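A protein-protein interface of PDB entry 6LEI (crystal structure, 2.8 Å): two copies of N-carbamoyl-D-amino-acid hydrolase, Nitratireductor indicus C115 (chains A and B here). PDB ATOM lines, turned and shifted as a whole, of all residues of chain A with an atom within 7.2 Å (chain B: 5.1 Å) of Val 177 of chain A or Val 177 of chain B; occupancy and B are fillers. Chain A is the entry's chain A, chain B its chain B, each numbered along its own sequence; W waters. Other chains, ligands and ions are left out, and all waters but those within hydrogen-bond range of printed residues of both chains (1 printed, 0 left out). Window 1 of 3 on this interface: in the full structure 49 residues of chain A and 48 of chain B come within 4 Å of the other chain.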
ATOM      1  N   HIS A 128      16.349  11.376 -27.346  1.00  0.00           N
ATOM      2  CA  HIS A 128      16.259  12.649 -28.061  1.00  0.00           C
ATOM      3  C   HIS A 128      17.656  13.248 -28.162  1.00  0.00           C
ATOM      4  O   HIS A 128      18.174  13.815 -27.199  1.00  0.00           O
ATOM      5  CB  HIS A 128      15.299  13.600 -27.357  1.00  0.00           C
ATOM      6  CG  HIS A 128      13.909  13.062 -27.219  1.00  0.00           C
ATOM      7  ND1 HIS A 128      13.493  12.351 -26.115  1.00  0.00           N
ATOM      8  CD2 HIS A 128      12.841  13.131 -28.048  1.00  0.00           C
ATOM      9  CE1 HIS A 128      12.227  12.005 -26.268  1.00  0.00           C
ATOM     10  NE2 HIS A 128      11.807  12.467 -27.432  1.00  0.00           N
ATOM     11  N   ASP A 173      16.011  15.339 -23.005  1.00  0.00           N
ATOM     12  CA  ASP A 173      14.823  14.511 -22.838  1.00  0.00           C
ATOM     13  C   ASP A 173      13.795  15.228 -21.981  1.00  0.00           C
ATOM     14  O   ASP A 173      12.587  15.113 -22.215  1.00  0.00           O
ATOM     15  CB  ASP A 173      15.177  13.164 -22.207  1.00  0.00           C
ATOM     16  CG  ASP A 173      15.799  12.198 -23.190  1.00  0.00           C
ATOM     17  OD1 ASP A 173      15.459  12.255 -24.390  1.00  0.00           O
ATOM     18  OD2 ASP A 173      16.629  11.373 -22.755  1.00  0.00           O
ATOM     19  N   ARG A 174      14.260  16.000 -20.995  1.00  0.00           N
ATOM     20  CA  ARG A 174      13.371  16.709 -20.086  1.00  0.00           C
ATOM     21  C   ARG A 174      12.567  17.802 -20.777  1.00  0.00           C
ATOM     22  O   ARG A 174      11.613  18.313 -20.182  1.00  0.00           O
ATOM     23  CB  ARG A 174      14.177  17.298 -18.924  1.00  0.00           C
ATOM     24  CG  ARG A 174      15.002  18.523 -19.267  1.00  0.00           C
ATOM     25  CD  ARG A 174      16.041  18.783 -18.184  1.00  0.00           C
ATOM     26  NE  ARG A 174      16.654  20.105 -18.295  1.00  0.00           N
ATOM     27  CZ  ARG A 174      17.653  20.403 -19.120  1.00  0.00           C
ATOM     28  NH1 ARG A 174      18.154  19.475 -19.924  1.00  0.00           N
ATOM     29  NH2 ARG A 174      18.145  21.633 -19.147  1.00  0.00           N
ATOM     30  N   ARG A 175      12.918  18.168 -22.013  1.00  0.00           N
ATOM     31  CA  ARG A 175      12.139  19.144 -22.763  1.00  0.00           C
ATOM     32  C   ARG A 175      10.899  18.541 -23.406  1.00  0.00           C
ATOM     33  O   ARG A 175       9.964  19.282 -23.731  1.00  0.00           O
ATOM     34  CB  ARG A 175      13.004  19.792 -23.851  1.00  0.00           C
ATOM     35  CG  ARG A 175      13.316  21.260 -23.610  1.00  0.00           C
ATOM     36  CD  ARG A 175      14.750  21.457 -23.147  1.00  0.00           C
ATOM     37  NE  ARG A 175      15.033  22.854 -22.831  1.00  0.00           N
ATOM     38  CZ  ARG A 175      16.232  23.314 -22.487  1.00  0.00           C
ATOM     39  NH1 ARG A 175      17.266  22.487 -22.418  1.00  0.00           N
ATOM     40  NH2 ARG A 175      16.398  24.602 -22.214  1.00  0.00           N
ATOM     41  N   TRP A 176      10.864  17.225 -23.592  1.00  0.00           N
ATOM     42  CA  TRP A 176       9.768  16.557 -24.281  1.00  0.00           C
ATOM     43  C   TRP A 176       8.823  15.925 -23.268  1.00  0.00           C
ATOM     44  O   TRP A 176       9.269  15.272 -22.319  1.00  0.00           O
ATOM     45  CB  TRP A 176      10.306  15.499 -25.246  1.00  0.00           C
ATOM     46  CG  TRP A 176      11.249  16.070 -26.257  1.00  0.00           C
ATOM     47  CD1 TRP A 176      12.608  16.145 -26.160  1.00  0.00           C
ATOM     48  CD2 TRP A 176      10.903  16.664 -27.514  1.00  0.00           C
ATOM     49  NE1 TRP A 176      13.129  16.742 -27.281  1.00  0.00           N
ATOM     50  CE2 TRP A 176      12.103  17.071 -28.127  1.00  0.00           C
ATOM     51  CE3 TRP A 176       9.695  16.889 -28.180  1.00  0.00           C
ATOM     52  CZ2 TRP A 176      12.131  17.689 -29.375  1.00  0.00           C
ATOM     53  CZ3 TRP A 176       9.724  17.502 -29.419  1.00  0.00           C
ATOM     54  CH2 TRP A 176      10.934  17.893 -30.004  1.00  0.00           C
ATOM     55  N   VAL A 177       7.518  16.125 -23.475  1.00  0.00           N
ATOM     56  CA  VAL A 177       6.527  15.572 -22.562  1.00  0.00           C
ATOM     57  C   VAL A 177       6.433  14.057 -22.678  1.00  0.00           C
ATOM     58  O   VAL A 177       6.018  13.393 -21.721  1.00  0.00           O
ATOM     59  CB  VAL A 177       5.149  16.218 -22.804  1.00  0.00           C
ATOM     60  CG1 VAL A 177       5.216  17.712 -22.548  1.00  0.00           C
ATOM     61  CG2 VAL A 177       4.666  15.934 -24.218  1.00  0.00           C
ATOM     62  N   GLU A 178       6.808  13.491 -23.828  1.00  0.00           N
ATOM     63  CA  GLU A 178       6.790  12.040 -23.973  1.00  0.00           C
ATOM     64  C   GLU A 178       7.765  11.371 -23.014  1.00  0.00           C
ATOM     65  O   GLU A 178       7.545  10.227 -22.602  1.00  0.00           O
ATOM     66  CB  GLU A 178       7.114  11.646 -25.415  1.00  0.00           C
ATOM     67  CG  GLU A 178       6.079  12.077 -26.446  1.00  0.00           C
ATOM     68  CD  GLU A 178       6.310  13.485 -26.968  1.00  0.00           C
ATOM     69  OE1 GLU A 178       7.137  14.215 -26.382  1.00  0.00           O
ATOM     70  OE2 GLU A 178       5.665  13.859 -27.971  1.00  0.00           O
ATOM     71  N   THR A 179       8.843  12.069 -22.647  1.00  0.00           N
ATOM     72  CA  THR A 179       9.809  11.511 -21.706  1.00  0.00           C
ATOM     73  C   THR A 179       9.154  11.213 -20.363  1.00  0.00           C
ATOM     74  O   THR A 179       9.322  10.123 -19.804  1.00  0.00           O
ATOM     75  CB  THR A 179      10.980  12.478 -21.530  1.00  0.00           C
ATOM     76  OG1 THR A 179      11.602  12.716 -22.799  1.00  0.00           O
ATOM     77  CG2 THR A 179      12.007  11.909 -20.568  1.00  0.00           C
ATOM     78  N   TYR A 180       8.390  12.170 -19.835  1.00  0.00           N
ATOM     79  CA  TYR A 180       7.753  11.985 -18.536  1.00  0.00           C
ATOM     80  C   TYR A 180       6.561  11.039 -18.620  1.00  0.00           C
ATOM     81  O   TYR A 180       6.351  10.221 -17.717  1.00  0.00           O
ATOM     82  CB  TYR A 180       7.312  13.335 -17.970  1.00  0.00           C
ATOM     83  CG  TYR A 180       8.421  14.354 -17.827  1.00  0.00           C
ATOM     84  CD1 TYR A 180       9.187  14.417 -16.670  1.00  0.00           C
ATOM     85  CD2 TYR A 180       8.693  15.262 -18.843  1.00  0.00           C
ATOM     86  CE1 TYR A 180      10.196  15.350 -16.532  1.00  0.00           C
ATOM     87  CE2 TYR A 180       9.701  16.198 -18.714  1.00  0.00           C
ATOM     88  CZ  TYR A 180      10.448  16.237 -17.556  1.00  0.00           C
ATOM     89  OH  TYR A 180      11.449  17.168 -17.420  1.00  0.00           O
ATOM     90  N   ARG A 181       5.771  11.134 -19.695  1.00  0.00           N
ATOM     91  CA  ARG A 181       4.528  10.371 -19.768  1.00  0.00           C
ATOM     92  C   ARG A 181       4.789   8.879 -19.924  1.00  0.00           C
ATOM     93  O   ARG A 181       4.122   8.060 -19.280  1.00  0.00           O
ATOM     94  CB  ARG A 181       3.664  10.879 -20.921  1.00  0.00           C
ATOM     95  CG  ARG A 181       2.346  10.137 -21.060  1.00  0.00           C
ATOM     96  CD  ARG A 181       1.170  11.036 -20.723  1.00  0.00           C
ATOM     97  NE  ARG A 181       1.341  11.716 -19.444  1.00  0.00           N
ATOM     98  CZ  ARG A 181       0.509  12.638 -18.971  1.00  0.00           C
ATOM     99  NH1 ARG A 181      -0.560  12.992 -19.672  1.00  0.00           N
ATOM    100  NH2 ARG A 181       0.745  13.206 -17.797  1.00  0.00           N
ATOM    101  N   VAL A 182       5.741   8.505 -20.783  1.00  0.00           N
ATOM    102  CA  VAL A 182       6.042   7.089 -20.994  1.00  0.00           C
ATOM    103  C   VAL A 182       6.437   6.431 -19.678  1.00  0.00           C
ATOM    104  O   VAL A 182       5.959   5.341 -19.339  1.00  0.00           O
ATOM    105  CB  VAL A 182       7.139   6.926 -22.062  1.00  0.00           C
ATOM    106  CG1 VAL A 182       7.666   5.499 -22.068  1.00  0.00           C
ATOM    107  CG2 VAL A 182       6.600   7.299 -23.433  1.00  0.00           C
ATOM    108  N   MET A 183       7.308   7.089 -18.912  1.00  0.00           N
ATOM    109  CA  MET A 183       7.640   6.580 -17.587  1.00  0.00           C
ATOM    110  C   MET A 183       6.483   6.768 -16.614  1.00  0.00           C
ATOM    111  O   MET A 183       6.275   5.925 -15.733  1.00  0.00           O
ATOM    112  CB  MET A 183       8.907   7.257 -17.068  1.00  0.00           C
ATOM    113  CG  MET A 183      10.162   6.838 -17.817  1.00  0.00           C
ATOM    114  SD  MET A 183      11.689   7.524 -17.151  1.00  0.00           S
ATOM    115  CE  MET A 183      11.569   9.227 -17.685  1.00  0.00           C
ATOM    116  N   THR A 218      10.137  22.849 -17.596  1.00  0.00           N
ATOM    117  CA  THR A 218       9.914  21.537 -18.191  1.00  0.00           C
ATOM    118  C   THR A 218       9.980  20.422 -17.152  1.00  0.00           C
ATOM    119  O   THR A 218       9.279  19.413 -17.286  1.00  0.00           O
ATOM    120  CB  THR A 218      10.931  21.288 -19.304  1.00  0.00           C
ATOM    121  OG1 THR A 218      12.258  21.416 -18.779  1.00  0.00           O
ATOM    122  CG2 THR A 218      10.740  22.288 -20.434  1.00  0.00           C
ATOM    123  N   ALA A 221       6.822  20.842 -14.589  1.00  0.00           N
ATOM    124  CA  ALA A 221       5.587  20.394 -15.222  1.00  0.00           C
ATOM    125  C   ALA A 221       5.573  18.880 -15.391  1.00  0.00           C
ATOM    126  O   ALA A 221       4.552  18.232 -15.134  1.00  0.00           O
ATOM    127  CB  ALA A 221       5.406  21.086 -16.569  1.00  0.00           C
ATOM    128  N   GLY A 222       6.694  18.300 -15.824  1.00  0.00           N
ATOM    129  CA  GLY A 222       6.767  16.855 -15.941  1.00  0.00           C
ATOM    130  C   GLY A 222       6.629  16.147 -14.608  1.00  0.00           C
ATOM    131  O   GLY A 222       6.092  15.037 -14.542  1.00  0.00           O
ATOM    132  N   GLN A 225       2.583  16.961 -13.666  1.00  0.00           N
ATOM    133  CA  GLN A 225       1.632  16.298 -14.549  1.00  0.00           C
ATOM    134  C   GLN A 225       1.789  14.783 -14.570  1.00  0.00           C
ATOM    135  O   GLN A 225       0.994  14.107 -15.230  1.00  0.00           O
ATOM    136  CB  GLN A 225       1.756  16.862 -15.965  1.00  0.00           C
ATOM    137  CG  GLN A 225       1.445  18.351 -16.048  1.00  0.00           C
ATOM    138  CD  GLN A 225       1.493  18.885 -17.464  1.00  0.00           C
ATOM    139  OE1 GLN A 225       2.541  19.321 -17.942  1.00  0.00           O
ATOM    140  NE2 GLN A 225       0.351  18.862 -18.144  1.00  0.00           N
ATOM    141  N   ASN A 226       2.784  14.235 -13.870  1.00  0.00           N
ATOM    142  CA  ASN A 226       2.919  12.796 -13.711  1.00  0.00           C
ATOM    143  C   ASN A 226       3.002  12.365 -12.255  1.00  0.00           C
ATOM    144  O   ASN A 226       3.117  11.163 -11.990  1.00  0.00           O
ATOM    145  CB  ASN A 226       4.153  12.281 -14.467  1.00  0.00           C
ATOM    146  CG  ASN A 226       4.005  12.401 -15.971  1.00  0.00           C
ATOM    147  OD1 ASN A 226       3.567  11.465 -16.639  1.00  0.00           O
ATOM    148  ND2 ASN A 226       4.363  13.561 -16.510  1.00  0.00           N
ATOM    149  N   TYR A 297      -5.223  10.498 -28.992  1.00  0.00           N
ATOM    150  CA  TYR A 297      -3.804  10.824 -28.924  1.00  0.00           C
ATOM    151  C   TYR A 297      -3.002  10.151 -30.034  1.00  0.00           C
ATOM    152  O   TYR A 297      -1.771  10.098 -29.954  1.00  0.00           O
ATOM    153  CB  TYR A 297      -3.224  10.430 -27.564  1.00  0.00           C
ATOM    154  CG  TYR A 297      -4.021  10.870 -26.352  1.00  0.00           C
ATOM    155  CD1 TYR A 297      -4.814  12.011 -26.380  1.00  0.00           C
ATOM    156  CD2 TYR A 297      -3.969  10.139 -25.171  1.00  0.00           C
ATOM    157  CE1 TYR A 297      -5.537  12.404 -25.267  1.00  0.00           C
ATOM    158  CE2 TYR A 297      -4.687  10.524 -24.057  1.00  0.00           C
ATOM    159  CZ  TYR A 297      -5.468  11.656 -24.109  1.00  0.00           C
ATOM    160  OH  TYR A 297      -6.182  12.038 -22.996  1.00  0.00           O
ATOM    161  N   ILE A 300       0.338  11.331 -31.665  1.00  0.00           N
ATOM    162  CA  ILE A 300       1.601  11.294 -30.935  1.00  0.00           C
ATOM    163  C   ILE A 300       2.464  10.126 -31.395  1.00  0.00           C
ATOM    164  O   ILE A 300       3.699  10.210 -31.370  1.00  0.00           O
ATOM    165  CB  ILE A 300       1.327  11.246 -29.419  1.00  0.00           C
ATOM    166  CG1 ILE A 300       0.474  12.445 -29.000  1.00  0.00           C
ATOM    167  CG2 ILE A 300       2.628  11.221 -28.630  1.00  0.00           C
ATOM    168  CD1 ILE A 300       0.195  12.512 -27.515  1.00  0.00           C
ATOM    169  N   ARG B 175      -4.673  20.234 -18.454  1.00  0.00           N
ATOM    170  CA  ARG B 175      -3.804  19.541 -17.513  1.00  0.00           C
ATOM    171  C   ARG B 175      -3.116  18.327 -18.121  1.00  0.00           C
ATOM    172  O   ARG B 175      -2.182  17.795 -17.511  1.00  0.00           O
ATOM    173  CB  ARG B 175      -4.600  19.108 -16.277  1.00  0.00           C
ATOM    174  CG  ARG B 175      -5.419  17.846 -16.477  1.00  0.00           C
ATOM    175  CD  ARG B 175      -6.466  17.684 -15.388  1.00  0.00           C
ATOM    176  NE  ARG B 175      -5.876  17.634 -14.054  1.00  0.00           N
ATOM    177  CZ  ARG B 175      -6.581  17.510 -12.933  1.00  0.00           C
ATOM    178  NH1 ARG B 175      -5.964  17.471 -11.759  1.00  0.00           N
ATOM    179  NH2 ARG B 175      -7.903  17.425 -12.986  1.00  0.00           N
ATOM    180  N   TRP B 176      -3.548  17.879 -19.296  1.00  0.00           N
ATOM    181  CA  TRP B 176      -2.967  16.719 -19.959  1.00  0.00           C
ATOM    182  C   TRP B 176      -2.031  17.179 -21.068  1.00  0.00           C
ATOM    183  O   TRP B 176      -2.418  17.984 -21.920  1.00  0.00           O
ATOM    184  CB  TRP B 176      -4.060  15.813 -20.528  1.00  0.00           C
ATOM    185  CG  TRP B 176      -5.024  15.333 -19.492  1.00  0.00           C
ATOM    186  CD1 TRP B 176      -6.305  15.764 -19.299  1.00  0.00           C
ATOM    187  CD2 TRP B 176      -4.781  14.338 -18.491  1.00  0.00           C
ATOM    188  NE1 TRP B 176      -6.876  15.094 -18.245  1.00  0.00           N
ATOM    189  CE2 TRP B 176      -5.961  14.213 -17.731  1.00  0.00           C
ATOM    190  CE3 TRP B 176      -3.681  13.538 -18.165  1.00  0.00           C
ATOM    191  CZ2 TRP B 176      -6.072  13.321 -16.665  1.00  0.00           C
ATOM    192  CZ3 TRP B 176      -3.794  12.653 -17.108  1.00  0.00           C
ATOM    193  CH2 TRP B 176      -4.980  12.552 -16.371  1.00  0.00           C
ATOM    194  N   VAL B 177      -0.799  16.660 -21.054  1.00  0.00           N
ATOM    195  CA  VAL B 177       0.190  17.046 -22.053  1.00  0.00           C
ATOM    196  C   VAL B 177      -0.226  16.617 -23.452  1.00  0.00           C
ATOM    197  O   VAL B 177       0.232  17.204 -24.438  1.00  0.00           O
ATOM    198  CB  VAL B 177       1.573  16.464 -21.694  1.00  0.00           C
ATOM    199  CG1 VAL B 177       2.056  17.024 -20.366  1.00  0.00           C
ATOM    200  CG2 VAL B 177       1.521  14.944 -21.651  1.00  0.00           C
ATOM    201  N   GLU B 178      -1.088  15.603 -23.565  1.00  0.00           N
ATOM    202  CA  GLU B 178      -1.530  15.152 -24.879  1.00  0.00           C
ATOM    203  C   GLU B 178      -2.380  16.205 -25.580  1.00  0.00           C
ATOM    204  O   GLU B 178      -2.424  16.241 -26.814  1.00  0.00           O
ATOM    205  CB  GLU B 178      -2.309  13.843 -24.758  1.00  0.00           C
ATOM    206  CG  GLU B 178      -1.507  12.675 -24.206  1.00  0.00           C
ATOM    207  CD  GLU B 178      -1.620  12.543 -22.701  1.00  0.00           C
ATOM    208  OE1 GLU B 178      -1.762  13.577 -22.017  1.00  0.00           O
ATOM    209  OE2 GLU B 178      -1.577  11.399 -22.202  1.00  0.00           O
ATOM    210  N   THR B 179      -3.058  17.063 -24.814  1.00  0.00           N
ATOM    211  CA  THR B 179      -3.883  18.107 -25.415  1.00  0.00           C
ATOM    212  C   THR B 179      -3.041  19.041 -26.276  1.00  0.00           C
ATOM    213  O   THR B 179      -3.382  19.317 -27.432  1.00  0.00           O
ATOM    214  CB  THR B 179      -4.608  18.894 -24.323  1.00  0.00           C
ATOM    215  OG1 THR B 179      -5.477  18.017 -23.593  1.00  0.00           O
ATOM    216  CG2 THR B 179      -5.425  20.027 -24.929  1.00  0.00           C
ATOM    217  N   TYR B 180      -1.928  19.531 -25.728  1.00  0.00           N
ATOM    218  CA  TYR B 180      -1.077  20.445 -26.481  1.00  0.00           C
ATOM    219  C   TYR B 180      -0.315  19.715 -27.581  1.00  0.00           C
ATOM    220  O   TYR B 180      -0.170  20.236 -28.693  1.00  0.00           O
ATOM    221  CB  TYR B 180      -0.099  21.148 -25.542  1.00  0.00           C
ATOM    222  CG  TYR B 180      -0.734  21.794 -24.333  1.00  0.00           C
ATOM    223  CD1 TYR B 180      -1.225  23.091 -24.392  1.00  0.00           C
ATOM    224  CD2 TYR B 180      -0.827  21.112 -23.126  1.00  0.00           C
ATOM    225  CE1 TYR B 180      -1.798  23.687 -23.287  1.00  0.00           C
ATOM    226  CE2 TYR B 180      -1.400  21.700 -22.017  1.00  0.00           C
ATOM    227  CZ  TYR B 180      -1.883  22.987 -22.103  1.00  0.00           C
ATOM    228  OH  TYR B 180      -2.452  23.579 -20.999  1.00  0.00           O
ATOM    229  N   ARG B 181       0.179  18.509 -27.289  1.00  0.00           N
ATOM    230  CA  ARG B 181       1.029  17.806 -28.243  1.00  0.00           C
ATOM    231  C   ARG B 181       0.249  17.376 -29.480  1.00  0.00           C
ATOM    232  O   ARG B 181       0.773  17.436 -30.599  1.00  0.00           O
ATOM    233  CB  ARG B 181       1.687  16.601 -27.568  1.00  0.00           C
ATOM    234  CG  ARG B 181       2.502  15.721 -28.505  1.00  0.00           C
ATOM    235  CD  ARG B 181       3.695  16.458 -29.103  1.00  0.00           C
ATOM    236  NE  ARG B 181       4.878  16.396 -28.246  1.00  0.00           N
ATOM    237  CZ  ARG B 181       5.381  17.431 -27.582  1.00  0.00           C
ATOM    238  NH1 ARG B 181       4.812  18.625 -27.676  1.00  0.00           N
ATOM    239  NH2 ARG B 181       6.461  17.274 -26.828  1.00  0.00           N
ATOM    240  N   VAL B 182      -1.002  16.942 -29.304  1.00  0.00           N
ATOM    241  CA  VAL B 182      -1.813  16.534 -30.449  1.00  0.00           C
ATOM    242  C   VAL B 182      -2.029  17.711 -31.392  1.00  0.00           C
ATOM    243  O   VAL B 182      -1.869  17.591 -32.612  1.00  0.00           O
ATOM    244  CB  VAL B 182      -3.149  15.931 -29.978  1.00  0.00           C
ATOM    245  CG1 VAL B 182      -4.153  15.908 -31.119  1.00  0.00           C
ATOM    246  CG2 VAL B 182      -2.932  14.525 -29.439  1.00  0.00           C
ATOM    247  N   GLN B 225       6.591  23.968 -24.616  1.00  0.00           N
ATOM    248  CA  GLN B 225       6.944  22.654 -25.144  1.00  0.00           C
ATOM    249  C   GLN B 225       6.289  22.356 -26.487  1.00  0.00           C
ATOM    250  O   GLN B 225       6.615  21.332 -27.101  1.00  0.00           O
ATOM    251  CB  GLN B 225       6.581  21.570 -24.129  1.00  0.00           C
ATOM    252  CG  GLN B 225       7.437  21.601 -22.871  1.00  0.00           C
ATOM    253  CD  GLN B 225       6.937  20.659 -21.795  1.00  0.00           C
ATOM    254  OE1 GLN B 225       5.776  20.722 -21.390  1.00  0.00           O
ATOM    255  NE2 GLN B 225       7.812  19.776 -21.327  1.00  0.00           N
HETATM  256  O   HOH W   1       8.182  19.273 -25.874  1.00  0.00           O
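Of the 19 printed residues of chain A, 9 touch a printed residue of chain B. Hydrophobic or aromatic side chains of chain A that line the printed part of chain B: Trp 176, Val 177, Tyr 297 and Ile 300. Along chain A the printed residues that touch a printed residue of chain B span positions 175 to 300. Of the 9 printed residues of chain B, 7 touch a printed residue of chain A. Printed residues of chain B that touch a printed residue of chain A: Arg 175, Trp 176, Val 177, Glu 178, Arg 181, Val 182 and Gln 225. Among the printed residues, 16 pairs touch across the chains. Among the printed residues, Asp or Glu carboxylates within 4 Å of a Lys or Arg side-chain nitrogen of the other chain: Glu 178 of chain A with Arg 181 of chain B (2.7 Å) and Arg 181 of chain A with Glu 178 of chain B (2.7 Å).
Among the printed residues, pairs that only touch across the chains: Trp 176 of chain A with Arg 181 of chain B (3.5 Å), Val 177 of chain A with Val 177 of chain B (3.8 Å), Val 177 of chain A with Arg 181 of chain B (3.4 Å), Val 177 of chain A with Gln 225 of chain B (3.3 Å), Arg 181 of chain A with Trp 176 of chain B (3.5 Å), Arg 181 of chain A with Val 177 of chain B (3.5 Å), Thr 218 of chain A with Gln 225 of chain B (3.96 Å), Gln 225 of chain A with Val 177 of chain B (3.4 Å), Tyr 297 of chain A with Glu 178 of chain B (3.5 Å), Tyr 297 of chain A with Val 182 of chain B (3.8 Å), Ile 300 of chain A with Glu 178 of chain B (3.7 Å) and Ile 300 of chain A with Arg 181 of chain B (3.9 Å).
Water W1 lies within hydrogen-bond range of O of Arg 175 of chain A, NH2 of Arg 181 of chain B and O of Gln 225 of chain B.
The side-chain amide nitrogen (NE2) of Gln 225 of chain B lies within hydrogen-bond range of the backbone carbonyl oxygen (O) of Arg 175 of chain A, 3.3 Å away. NH1 of Arg 181 of chain A lies within salt-bridge range of OE1 of Glu 178 of chain B (2.7 Å). O of Arg 175 of chain B lies within hydrogen-bond range of NE2 of Gln 225 of chain A (2.8 Å). The side-chain carboxylate (OE2) of Glu 178 of chain A is in salt-bridge range of the guanidinium group (NE) of Arg 181 of chain B (2.7 Å).
Asp 173 of chain A touches none of the printed residues of chain B. Of the printed residues of chain B, Trp 176 of chain A touches Arg 181. Val 177 of chain A touches just these residues of chain B: Val 177 (3.8 Å), Arg 181 (3.4 Å) and Gln 225 (3.3 Å). Of the printed residues of chain B, Glu 178 of chain A touches Arg 181. Met 183 of chain A touches none of the printed residues of chain B. Of the printed residues of chain B, Gln 225 of chain A touches Arg 175 and Val 177. Printed residues of chain B within 4 Å of Ile 300 of chain A: Glu 178 (3.7 Å) and Arg 181 (3.9 Å). Printed residues of chain A within 4 Å of Glu 178 of chain B: Arg 181, Tyr 297 and Ile 300. The nearest printed residue of chain A that does not touch Arg 181 of chain B is Arg 175 of chain A (5.1 Å).
OG1 of Thr 218 of chain A sits close to O of Arg 174 of chain A, 3.5 Å away. O of Trp 176 of chain A sits close to OG1 of Thr 179 of chain A. The backbone carbonyl oxygen of Gln 225 of chain B is in hydrogen-bond range of the guanidinium group of Arg 181 of chain B, at 3.3 Å. The side-chain hydroxyl of Tyr 180 of chain A lies within hydrogen-bond range of the backbone carbonyl oxygen of Thr 218 of chain A (3.1 Å). The backbone carbonyl oxygen of Trp 176 of chain B sits close to the side-chain hydroxyl of Thr 179 of chain B. O of Gln 225 of chain A sits at hydrogen-bond distance from NH2 of Arg 181 of chain A, 2.7 Å away.
Arg 175 of chain A touches Gln 225 of chain B, and with the chains exchanged Gln 225 of chain A touches Arg 175 of chain B. Trp 176 of chain A touches Arg 181 of chain B, and with the chains exchanged Arg 181 of chain A touches Trp 176 of chain B. Val 177 of chain A touches Gln 225 of chain B, and with the chains exchanged Gln 225 of chain A touches Val 177 of chain B. Glu 178 of chain A touches Arg 181 of chain B, and with the chains exchanged Arg 181 of chain A touches Glu 178 of chain B. Positions printed for both chains: 175, 176, 177, 178, 179, 180, 181, 182 and 225. Of the 16 pairs that touch across the chains among the printed residues, 11 have their exchanged pair printed and touching as well.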
